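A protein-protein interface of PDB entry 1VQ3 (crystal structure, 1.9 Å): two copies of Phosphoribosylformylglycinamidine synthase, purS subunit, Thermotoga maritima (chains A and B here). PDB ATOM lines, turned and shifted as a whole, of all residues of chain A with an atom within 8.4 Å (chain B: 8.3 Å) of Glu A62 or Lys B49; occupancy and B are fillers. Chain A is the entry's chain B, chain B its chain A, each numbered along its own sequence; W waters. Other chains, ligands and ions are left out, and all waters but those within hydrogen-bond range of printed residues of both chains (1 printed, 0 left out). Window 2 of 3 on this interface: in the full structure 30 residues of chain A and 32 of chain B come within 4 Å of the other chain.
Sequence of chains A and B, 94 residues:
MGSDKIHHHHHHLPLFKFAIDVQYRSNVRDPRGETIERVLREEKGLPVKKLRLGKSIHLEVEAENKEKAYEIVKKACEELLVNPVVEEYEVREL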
ATOM      1  N   HIS A  11      -8.472  -8.468  35.025  1.00  0.00           N
ATOM      2  CA  HIS A  11      -8.038  -7.376  34.089  1.00  0.00           C
ATOM      3  C   HIS A  11      -8.869  -7.375  32.811  1.00  0.00           C
ATOM      4  O   HIS A  11      -8.864  -8.361  32.062  1.00  0.00           O
ATOM      5  CB  HIS A  11      -6.554  -7.501  33.713  1.00  0.00           C
ATOM      6  CG  HIS A  11      -5.617  -7.119  34.813  1.00  0.00           C
ATOM      7  ND1 HIS A  11      -5.792  -5.989  35.580  1.00  0.00           N
ATOM      8  CE1 HIS A  11      -4.812  -5.933  36.466  1.00  0.00           C
ATOM      9  N   HIS A  12      -9.559  -6.260  32.567  1.00  0.00           N
ATOM     10  CA  HIS A  12     -10.356  -6.077  31.365  1.00  0.00           C
ATOM     11  C   HIS A  12      -9.421  -5.387  30.397  1.00  0.00           C
ATOM     12  O   HIS A  12      -9.079  -4.210  30.575  1.00  0.00           O
ATOM     13  CB  HIS A  12     -11.576  -5.191  31.644  1.00  0.00           C
ATOM     14  CG  HIS A  12     -12.539  -5.088  30.490  1.00  0.00           C
ATOM     15  ND1 HIS A  12     -12.403  -5.828  29.331  1.00  0.00           N
ATOM     16  CD2 HIS A  12     -13.681  -4.376  30.339  1.00  0.00           C
ATOM     17  CE1 HIS A  12     -13.399  -5.553  28.505  1.00  0.00           C
ATOM     18  NE2 HIS A  12     -14.190  -4.674  29.088  1.00  0.00           N
ATOM     19  N   LEU A  13      -9.006  -6.113  29.371  1.00  0.00           N
ATOM     20  CA  LEU A  13      -8.044  -5.600  28.417  1.00  0.00           C
ATOM     21  C   LEU A  13      -8.723  -4.887  27.224  1.00  0.00           C
ATOM     22  O   LEU A  13      -9.827  -5.250  26.817  1.00  0.00           O
ATOM     23  CB  LEU A  13      -7.207  -6.750  27.876  1.00  0.00           C
ATOM     24  CG  LEU A  13      -5.834  -7.097  28.494  1.00  0.00           C
ATOM     25  CD1 LEU A  13      -5.578  -6.518  29.842  1.00  0.00           C
ATOM     26  CD2 LEU A  13      -5.664  -8.560  28.480  1.00  0.00           C
ATOM     27  N   PRO A  14      -8.035  -3.910  26.649  1.00  0.00           N
ATOM     28  CA  PRO A  14      -8.538  -3.246  25.443  1.00  0.00           C
ATOM     29  C   PRO A  14      -8.562  -4.214  24.255  1.00  0.00           C
ATOM     30  O   PRO A  14      -7.798  -5.188  24.205  1.00  0.00           O
ATOM     31  CB  PRO A  14      -7.583  -2.091  25.231  1.00  0.00           C
ATOM     32  CG  PRO A  14      -6.333  -2.439  26.028  1.00  0.00           C
ATOM     33  CD  PRO A  14      -6.711  -3.379  27.065  1.00  0.00           C
ATOM     34  N   LEU A  15      -9.468  -3.936  23.343  1.00  0.00           N
ATOM     35  CA  LEU A  15      -9.676  -4.720  22.152  1.00  0.00           C
ATOM     36  C   LEU A  15      -8.926  -4.073  21.010  1.00  0.00           C
ATOM     37  O   LEU A  15      -8.855  -2.820  20.916  1.00  0.00           O
ATOM     38  CB  LEU A  15     -11.175  -4.730  21.872  1.00  0.00           C
ATOM     39  CG  LEU A  15     -11.856  -5.602  20.845  1.00  0.00           C
ATOM     40  CD1 LEU A  15     -11.686  -7.056  21.149  1.00  0.00           C
ATOM     41  CD2 LEU A  15     -13.323  -5.250  20.841  1.00  0.00           C
ATOM     42  N   PHE A  16      -8.373  -4.926  20.144  1.00  0.00           N
ATOM     43  CA  PHE A  16      -7.619  -4.521  18.951  1.00  0.00           C
ATOM     44  C   PHE A  16      -8.186  -5.254  17.756  1.00  0.00           C
ATOM     45  O   PHE A  16      -8.261  -6.477  17.750  1.00  0.00           O
ATOM     46  CB  PHE A  16      -6.139  -4.824  19.100  1.00  0.00           C
ATOM     47  CG  PHE A  16      -5.494  -4.085  20.231  1.00  0.00           C
ATOM     48  CD1 PHE A  16      -5.581  -4.574  21.516  1.00  0.00           C
ATOM     49  CD2 PHE A  16      -4.837  -2.883  20.003  1.00  0.00           C
ATOM     50  CE1 PHE A  16      -5.022  -3.899  22.566  1.00  0.00           C
ATOM     51  CE2 PHE A  16      -4.282  -2.183  21.056  1.00  0.00           C
ATOM     52  CZ  PHE A  16      -4.382  -2.684  22.349  1.00  0.00           C
ATOM     53  N   LYS A  17      -8.666  -4.517  16.762  1.00  0.00           N
ATOM     54  CA  LYS A  17      -9.296  -5.118  15.616  1.00  0.00           C
ATOM     55  C   LYS A  17      -8.393  -5.054  14.367  1.00  0.00           C
ATOM     56  O   LYS A  17      -7.769  -3.997  14.039  1.00  0.00           O
ATOM     57  CB  LYS A  17     -10.670  -4.495  15.340  1.00  0.00           C
ATOM     58  CG  LYS A  17     -11.528  -4.299  16.609  1.00  0.00           C
ATOM     59  CD  LYS A  17     -12.861  -3.750  16.265  1.00  0.00           C
ATOM     60  CE  LYS A  17     -13.737  -3.638  17.520  1.00  0.00           C
ATOM     61  NZ  LYS A  17     -15.001  -2.943  17.235  1.00  0.00           N
ATOM     62  N   PHE A  18      -8.371  -6.171  13.636  1.00  0.00           N
ATOM     63  CA  PHE A  18      -7.457  -6.302  12.483  1.00  0.00           C
ATOM     64  C   PHE A  18      -8.098  -6.974  11.272  1.00  0.00           C
ATOM     65  O   PHE A  18      -9.078  -7.753  11.414  1.00  0.00           O
ATOM     66  CB  PHE A  18      -6.223  -7.157  12.871  1.00  0.00           C
ATOM     67  CG  PHE A  18      -5.364  -6.559  13.929  1.00  0.00           C
ATOM     68  CD1 PHE A  18      -4.439  -5.559  13.621  1.00  0.00           C
ATOM     69  CD2 PHE A  18      -5.407  -7.037  15.198  1.00  0.00           C
ATOM     70  CE1 PHE A  18      -3.612  -5.033  14.641  1.00  0.00           C
ATOM     71  CE2 PHE A  18      -4.591  -6.525  16.194  1.00  0.00           C
ATOM     72  CZ  PHE A  18      -3.712  -5.540  15.918  1.00  0.00           C
ATOM     73  N   ILE A  57      -8.853 -12.347   6.538  1.00  0.00           N
ATOM     74  CA  ILE A  57      -9.257 -12.764   7.883  1.00  0.00           C
ATOM     75  C   ILE A  57      -9.400 -11.491   8.732  1.00  0.00           C
ATOM     76  O   ILE A  57      -8.436 -10.796   9.013  1.00  0.00           O
ATOM     77  CB  ILE A  57      -8.256 -13.741   8.526  1.00  0.00           C
ATOM     78  CG1 ILE A  57      -7.997 -14.960   7.646  1.00  0.00           C
ATOM     79  CG2 ILE A  57      -8.733 -14.172   9.876  1.00  0.00           C
ATOM     80  CD1 ILE A  57      -6.709 -14.984   6.879  1.00  0.00           C
ATOM     81  N   HIS A  58     -10.629 -11.211   9.132  1.00  0.00           N
ATOM     82  CA  HIS A  58     -10.911 -10.186  10.139  1.00  0.00           C
ATOM     83  C   HIS A  58     -10.976 -10.885  11.498  1.00  0.00           C
ATOM     84  O   HIS A  58     -11.524 -11.989  11.638  1.00  0.00           O
ATOM     85  CB  HIS A  58     -12.251  -9.519   9.869  1.00  0.00           C
ATOM     86  CG  HIS A  58     -12.281  -8.703   8.621  1.00  0.00           C
ATOM     87  ND1 HIS A  58     -13.292  -7.819   8.347  1.00  0.00           N
ATOM     88  CD2 HIS A  58     -11.463  -8.684   7.548  1.00  0.00           C
ATOM     89  CE1 HIS A  58     -13.069  -7.239   7.176  1.00  0.00           C
ATOM     90  NE2 HIS A  58     -11.955  -7.738   6.670  1.00  0.00           N
ATOM     91  N   LEU A  59     -10.334 -10.268  12.483  1.00  0.00           N
ATOM     92  CA  LEU A  59     -10.376 -10.795  13.828  1.00  0.00           C
ATOM     93  C   LEU A  59     -10.046  -9.682  14.814  1.00  0.00           C
ATOM     94  O   LEU A  59      -9.524  -8.623  14.442  1.00  0.00           O
ATOM     95  CB  LEU A  59      -9.455 -11.988  14.025  1.00  0.00           C
ATOM     96  CG  LEU A  59      -7.972 -11.816  13.725  1.00  0.00           C
ATOM     97  CD1 LEU A  59      -7.229 -10.936  14.656  1.00  0.00           C
ATOM     98  CD2 LEU A  59      -7.426 -13.200  13.776  1.00  0.00           C
ATOM     99  N   GLU A  60     -10.497  -9.891  16.034  1.00  0.00           N
ATOM    100  CA  GLU A  60     -10.305  -8.963  17.164  1.00  0.00           C
ATOM    101  C   GLU A  60      -9.530  -9.727  18.253  1.00  0.00           C
ATOM    102  O   GLU A  60      -9.727 -10.956  18.470  1.00  0.00           O
ATOM    103  CB  GLU A  60     -11.660  -8.580  17.729  1.00  0.00           C
ATOM    104  CG  GLU A  60     -12.630  -8.268  16.605  1.00  0.00           C
ATOM    105  CD  GLU A  60     -13.873  -7.558  17.072  1.00  0.00           C
ATOM    106  OE1 GLU A  60     -14.193  -7.649  18.269  1.00  0.00           O
ATOM    107  OE2 GLU A  60     -14.519  -6.911  16.209  1.00  0.00           O
ATOM    108  N   VAL A  61      -8.620  -9.025  18.896  1.00  0.00           N
ATOM    109  CA  VAL A  61      -7.788  -9.572  19.941  1.00  0.00           C
ATOM    110  C   VAL A  61      -7.900  -8.708  21.216  1.00  0.00           C
ATOM    111  O   VAL A  61      -7.943  -7.479  21.149  1.00  0.00           O
ATOM    112  CB  VAL A  61      -6.306  -9.598  19.454  1.00  0.00           C
ATOM    113  CG1 VAL A  61      -5.364  -9.775  20.597  1.00  0.00           C
ATOM    114  CG2 VAL A  61      -6.112 -10.718  18.471  1.00  0.00           C
ATOM    115  N   GLU A  62      -7.924  -9.342  22.385  1.00  0.00           N
ATOM    116  CA  GLU A  62      -7.674  -8.616  23.630  1.00  0.00           C
ATOM    117  C   GLU A  62      -6.208  -8.724  24.054  1.00  0.00           C
ATOM    118  O   GLU A  62      -5.607  -9.805  24.030  1.00  0.00           O
ATOM    119  CB  GLU A  62      -8.580  -9.110  24.742  1.00  0.00           C
ATOM    120  CG  GLU A  62      -9.757  -8.208  25.007  1.00  0.00           C
ATOM    121  CD  GLU A  62     -10.674  -8.785  26.076  1.00  0.00           C
ATOM    122  OE1 GLU A  62     -10.227  -8.958  27.239  1.00  0.00           O
ATOM    123  OE2 GLU A  62     -11.825  -9.090  25.725  1.00  0.00           O
ATOM    124  N   ALA A  63      -5.609  -7.600  24.435  1.00  0.00           N
ATOM    125  CA  ALA A  63      -4.201  -7.603  24.750  1.00  0.00           C
ATOM    126  C   ALA A  63      -3.852  -6.379  25.621  1.00  0.00           C
ATOM    127  O   ALA A  63      -4.650  -5.464  25.745  1.00  0.00           O
ATOM    128  CB  ALA A  63      -3.397  -7.586  23.483  1.00  0.00           C
ATOM    129  N   GLU A  64      -2.648  -6.396  26.187  1.00  0.00           N
ATOM    130  CA  GLU A  64      -2.221  -5.387  27.148  1.00  0.00           C
ATOM    131  C   GLU A  64      -1.863  -4.065  26.469  1.00  0.00           C
ATOM    132  O   GLU A  64      -1.979  -2.987  27.073  1.00  0.00           O
ATOM    133  CB  GLU A  64      -1.050  -5.931  27.993  1.00  0.00           C
ATOM    134  CG  GLU A  64      -1.421  -7.124  28.862  1.00  0.00           C
ATOM    135  N   ASN A  65      -1.443  -4.137  25.207  1.00  0.00           N
ATOM    136  CA  ASN A  65      -1.097  -2.952  24.441  1.00  0.00           C
ATOM    137  C   ASN A  65      -1.020  -3.319  22.959  1.00  0.00           C
ATOM    138  O   ASN A  65      -1.224  -4.468  22.602  1.00  0.00           O
ATOM    139  CB  ASN A  65       0.233  -2.384  24.940  1.00  0.00           C
ATOM    140  CG  ASN A  65       1.362  -3.389  24.856  1.00  0.00           C
ATOM    141  OD1 ASN A  65       1.666  -3.893  23.781  1.00  0.00           O
ATOM    142  ND2 ASN A  65       1.993  -3.689  25.996  1.00  0.00           N
ATOM    143  N   LYS A  68       1.820  -6.089  21.892  1.00  0.00           N
ATOM    144  CA  LYS A  68       1.388  -7.435  22.230  1.00  0.00           C
ATOM    145  C   LYS A  68       0.262  -7.865  21.264  1.00  0.00           C
ATOM    146  O   LYS A  68       0.202  -9.011  20.855  1.00  0.00           O
ATOM    147  CB  LYS A  68       0.836  -7.487  23.647  1.00  0.00           C
ATOM    148  CG  LYS A  68       1.826  -7.157  24.769  1.00  0.00           C
ATOM    149  CD  LYS A  68       2.776  -8.305  25.066  1.00  0.00           C
ATOM    150  CE  LYS A  68       3.969  -7.844  25.942  1.00  0.00           C
ATOM    151  NZ  LYS A  68       3.522  -6.855  26.968  1.00  0.00           N
ATOM    152  N   ALA A  69      -0.635  -6.948  20.889  1.00  0.00           N
ATOM    153  CA  ALA A  69      -1.710  -7.368  20.000  1.00  0.00           C
ATOM    154  C   ALA A  69      -1.167  -7.817  18.643  1.00  0.00           C
ATOM    155  O   ALA A  69      -1.602  -8.841  18.129  1.00  0.00           O
ATOM    156  CB  ALA A  69      -2.807  -6.257  19.844  1.00  0.00           C
ATOM    157  N   ILE A  72       0.245 -11.232  18.856  1.00  0.00           N
ATOM    158  CA  ILE A  72      -0.838 -12.219  18.744  1.00  0.00           C
ATOM    159  C   ILE A  72      -1.245 -12.476  17.288  1.00  0.00           C
ATOM    160  O   ILE A  72      -1.377 -13.636  16.859  1.00  0.00           O
ATOM    161  CB  ILE A  72      -2.054 -11.816  19.617  1.00  0.00           C
ATOM    162  CG1 ILE A  72      -1.638 -11.853  21.095  1.00  0.00           C
ATOM    163  CG2 ILE A  72      -3.265 -12.789  19.355  1.00  0.00           C
ATOM    164  CD1 ILE A  72      -2.548 -11.169  22.054  1.00  0.00           C
ATOM    165  N   GLU B  37     -11.345 -20.057  14.284  1.00  0.00           N
ATOM    166  CA  GLU B  37     -11.343 -19.327  15.556  1.00  0.00           C
ATOM    167  C   GLU B  37     -11.177 -20.269  16.749  1.00  0.00           C
ATOM    168  O   GLU B  37     -10.404 -19.989  17.680  1.00  0.00           O
ATOM    169  CB  GLU B  37     -12.654 -18.567  15.726  1.00  0.00           C
ATOM    170  CG  GLU B  37     -12.685 -17.762  17.006  1.00  0.00           C
ATOM    171  CD  GLU B  37     -13.928 -16.919  17.141  1.00  0.00           C
ATOM    172  OE1 GLU B  37     -14.397 -16.332  16.129  1.00  0.00           O
ATOM    173  OE2 GLU B  37     -14.422 -16.824  18.283  1.00  0.00           O
ATOM    174  N   LEU B  40      -7.535 -21.351  16.858  1.00  0.00           N
ATOM    175  CA  LEU B  40      -6.639 -20.320  17.385  1.00  0.00           C
ATOM    176  C   LEU B  40      -6.823 -20.164  18.910  1.00  0.00           C
ATOM    177  O   LEU B  40      -5.842 -19.999  19.644  1.00  0.00           O
ATOM    178  CB  LEU B  40      -6.902 -18.979  16.702  1.00  0.00           C
ATOM    179  CG  LEU B  40      -6.433 -18.850  15.227  1.00  0.00           C
ATOM    180  CD1 LEU B  40      -6.841 -17.516  14.602  1.00  0.00           C
ATOM    181  CD2 LEU B  40      -4.913 -19.050  15.112  1.00  0.00           C
ATOM    182  N   ARG B  41      -8.060 -20.226  19.376  1.00  0.00           N
ATOM    183  CA  ARG B  41      -8.354 -20.059  20.798  1.00  0.00           C
ATOM    184  C   ARG B  41      -7.982 -21.294  21.607  1.00  0.00           C
ATOM    185  O   ARG B  41      -7.222 -21.225  22.565  1.00  0.00           O
ATOM    186  CB  ARG B  41      -9.837 -19.771  21.029  1.00  0.00           C
ATOM    187  CG  ARG B  41     -10.346 -18.417  20.636  1.00  0.00           C
ATOM    188  CD  ARG B  41     -11.765 -18.176  21.176  1.00  0.00           C
ATOM    189  NE  ARG B  41     -11.728 -17.918  22.615  1.00  0.00           N
ATOM    190  N   LEU B  46      -4.583 -18.544  21.774  1.00  0.00           N
ATOM    191  CA  LEU B  46      -4.530 -17.111  21.472  1.00  0.00           C
ATOM    192  C   LEU B  46      -5.849 -16.391  21.826  1.00  0.00           C
ATOM    193  O   LEU B  46      -6.907 -16.875  21.491  1.00  0.00           O
ATOM    194  CB  LEU B  46      -4.159 -16.886  20.016  1.00  0.00           C
ATOM    195  CG  LEU B  46      -2.815 -17.523  19.633  1.00  0.00           C
ATOM    196  CD1 LEU B  46      -2.673 -17.645  18.147  1.00  0.00           C
ATOM    197  CD2 LEU B  46      -1.630 -16.773  20.209  1.00  0.00           C
ATOM    198  N   PRO B  47      -5.765 -15.210  22.429  1.00  0.00           N
ATOM    199  CA  PRO B  47      -6.954 -14.446  22.820  1.00  0.00           C
ATOM    200  C   PRO B  47      -7.661 -13.746  21.613  1.00  0.00           C
ATOM    201  O   PRO B  47      -7.654 -12.512  21.542  1.00  0.00           O
ATOM    202  CB  PRO B  47      -6.384 -13.421  23.805  1.00  0.00           C
ATOM    203  CG  PRO B  47      -5.013 -13.198  23.368  1.00  0.00           C
ATOM    204  CD  PRO B  47      -4.512 -14.493  22.788  1.00  0.00           C
ATOM    205  N   VAL B  48      -8.178 -14.546  20.667  1.00  0.00           N
ATOM    206  CA  VAL B  48      -8.814 -14.065  19.422  1.00  0.00           C
ATOM    207  C   VAL B  48     -10.323 -14.260  19.435  1.00  0.00           C
ATOM    208  O   VAL B  48     -10.828 -15.278  19.972  1.00  0.00           O
ATOM    209  CB  VAL B  48      -8.292 -14.818  18.211  1.00  0.00           C
ATOM    210  CG1 VAL B  48      -9.196 -14.609  17.012  1.00  0.00           C
ATOM    211  CG2 VAL B  48      -6.912 -14.390  17.881  1.00  0.00           C
ATOM    212  N   LYS B  49     -11.042 -13.309  18.821  1.00  0.00           N
ATOM    213  CA  LYS B  49     -12.516 -13.341  18.743  1.00  0.00           C
ATOM    214  C   LYS B  49     -12.987 -12.834  17.407  1.00  0.00           C
ATOM    215  O   LYS B  49     -12.214 -12.258  16.598  1.00  0.00           O
ATOM    216  CB  LYS B  49     -13.195 -12.428  19.801  1.00  0.00           C
ATOM    217  CG  LYS B  49     -12.984 -12.788  21.222  1.00  0.00           C
ATOM    218  CD  LYS B  49     -12.588 -11.568  22.092  1.00  0.00           C
ATOM    219  CE  LYS B  49     -12.022 -12.048  23.455  1.00  0.00           C
ATOM    220  NZ  LYS B  49     -11.334 -10.989  24.253  1.00  0.00           N
ATOM    221  N   LYS B  50     -14.254 -13.150  17.169  1.00  0.00           N
ATOM    222  CA  LYS B  50     -15.049 -12.654  16.070  1.00  0.00           C
ATOM    223  C   LYS B  50     -14.319 -12.820  14.758  1.00  0.00           C
ATOM    224  O   LYS B  50     -14.238 -11.905  13.955  1.00  0.00           O
ATOM    225  CB  LYS B  50     -15.435 -11.196  16.323  1.00  0.00           C
ATOM    226  CG  LYS B  50     -16.121 -11.056  17.651  1.00  0.00           C
ATOM    227  CD  LYS B  50     -17.069  -9.930  17.644  1.00  0.00           C
ATOM    228  CE  LYS B  50     -17.698  -9.726  19.012  1.00  0.00           C
ATOM    229  NZ  LYS B  50     -18.325  -8.393  19.010  1.00  0.00           N
ATOM    230  N   LEU B  51     -13.781 -14.004  14.544  1.00  0.00           N
ATOM    231  CA  LEU B  51     -12.996 -14.253  13.361  1.00  0.00           C
ATOM    232  C   LEU B  51     -13.932 -14.413  12.183  1.00  0.00           C
ATOM    233  O   LEU B  51     -14.879 -15.204  12.255  1.00  0.00           O
ATOM    234  CB  LEU B  51     -12.169 -15.514  13.552  1.00  0.00           C
ATOM    235  CG  LEU B  51     -11.085 -15.671  12.490  1.00  0.00           C
ATOM    236  CD1 LEU B  51      -9.815 -16.115  13.082  1.00  0.00           C
ATOM    237  CD2 LEU B  51     -11.494 -16.538  11.381  1.00  0.00           C
ATOM    238  N   ARG B  52     -13.609 -13.737  11.067  1.00  0.00           N
ATOM    239  CA  ARG B  52     -14.309 -13.956   9.820  1.00  0.00           C
ATOM    240  C   ARG B  52     -13.347 -14.197   8.706  1.00  0.00           C
ATOM    241  O   ARG B  52     -12.419 -13.462   8.516  1.00  0.00           O
ATOM    242  CB  ARG B  52     -15.188 -12.786   9.515  1.00  0.00           C
ATOM    243  CG  ARG B  52     -16.175 -12.551  10.611  1.00  0.00           C
ATOM    244  CD  ARG B  52     -17.284 -11.700  10.184  1.00  0.00           C
ATOM    245  NE  ARG B  52     -16.788 -10.462   9.608  1.00  0.00           N
ATOM    246  CZ  ARG B  52     -17.429  -9.738   8.698  1.00  0.00           C
ATOM    247  NH1 ARG B  52     -18.644 -10.102   8.251  1.00  0.00           N
ATOM    248  NH2 ARG B  52     -16.866  -8.610   8.263  1.00  0.00           N
HETATM  249  O   HOH W   1     -16.510  -6.120  18.797  1.00  0.00           O
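The backbone NH (N) of Glu A62 sits at hydrogen-bond distance from the backbone carbonyl oxygen (O) of Pro B47 (3.3 Å).
The backbone carbonyl oxygen (O) of Glu A60 sits at hydrogen-bond distance from the backbone NH (N) of Lys B49, 2.7 Å away.
NZ of Lys B49 is in salt-bridge range of OE2 of Glu A62, at 2.5 Å.
The backbone NH (N) of Arg B52 sits at hydrogen-bond distance from the backbone carbonyl oxygen (O) of His A58 (2.8 Å).
The side-chain carboxylate (OE1) of Glu B37 lies within hydrogen-bond range of the backbone NH (N) of Lys B50, at 3.4 Å.
The backbone NH (N) of Leu B51 lies within hydrogen-bond range of the side-chain carboxylate (OE1) of Glu B37.
O of Val A61 sits at hydrogen-bond distance from N of Phe A16 (2.8 Å).
N of Phe A18 sits at hydrogen-bond distance from O of Leu A59, 2.8 Å away.
Ile A57 touches Leu B51 (CG2 to CG, 3.8 Å).
His A58 touches Lys B50 (O to O, 3.6 Å).
O of His A58 touches CA of Leu B51, 3.2 Å away.
Leu A59 touches Val B48 (CD2 to CG1, 3.9 Å).
Leu A59 touches Lys B49.
Leu B51 touches Leu A59.
Glu A60 touches Val B48.
O of Pro B47 touches CA of Val A61 (3.4 Å).
Val B48 touches Val A61.
Ile A72 touches Pro B47.
Of chain B, only Pro B47 (3.3 Å) and Lys B49 (2.5 Å) come within 4 Å of Glu A62.
Of the printed residues of chain B, Glu A60 touches Val B48, Lys B49 and Lys B50.
Printed residues of chain B within 4 Å of Ile A72: Pro B47 (3.5 Å).
Of the printed residues of chain A, Leu B51 touches Ile A57, His A58 and Leu A59.
Phe A16 touches none of the printed residues of chain B.
Asn A65 touches none of the printed residues of chain B.
The nearest residue of chain B that does not touch Glu A62 is Val B48 (5.5 Å).
The nearest residue of chain A that does not touch Lys B49 is Leu A15 (4.7 Å).
The nearest printed residue of chain B that does not touch Val A61 is Lys B49 (4.9 Å).
Of the 10 printed residues of chain B, 6 touch a printed residue of chain A.
Printed residues of chain B that touch a printed residue of chain A: Pro B47, Val B48, Lys B49, Lys B50, Leu B51 and Arg B52.
Of the 20 printed residues of chain A, 7 touch a printed residue of chain B.
Printed residues of chain A that touch a printed residue of chain B: Ile A57, His A58, Leu A59, Glu A60, Val A61, Glu A62 and Ile A72.
Hydrophobic or aromatic side chains of chain A that line the printed part of chain B: Ile A57, His A58, Leu A59, Val A61 and Ile A72.
Among the printed residues, 16 pairs touch across the chains.
No position is printed for both chains.
Of the 16 pairs that touch across the chains among the printed residues, none has its exchanged pair printed and touching as well.
Water W1 bridges the side-chain carboxylate (OE1) of Glu A60 and the side-chain amino group (NZ) of Lys B50.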
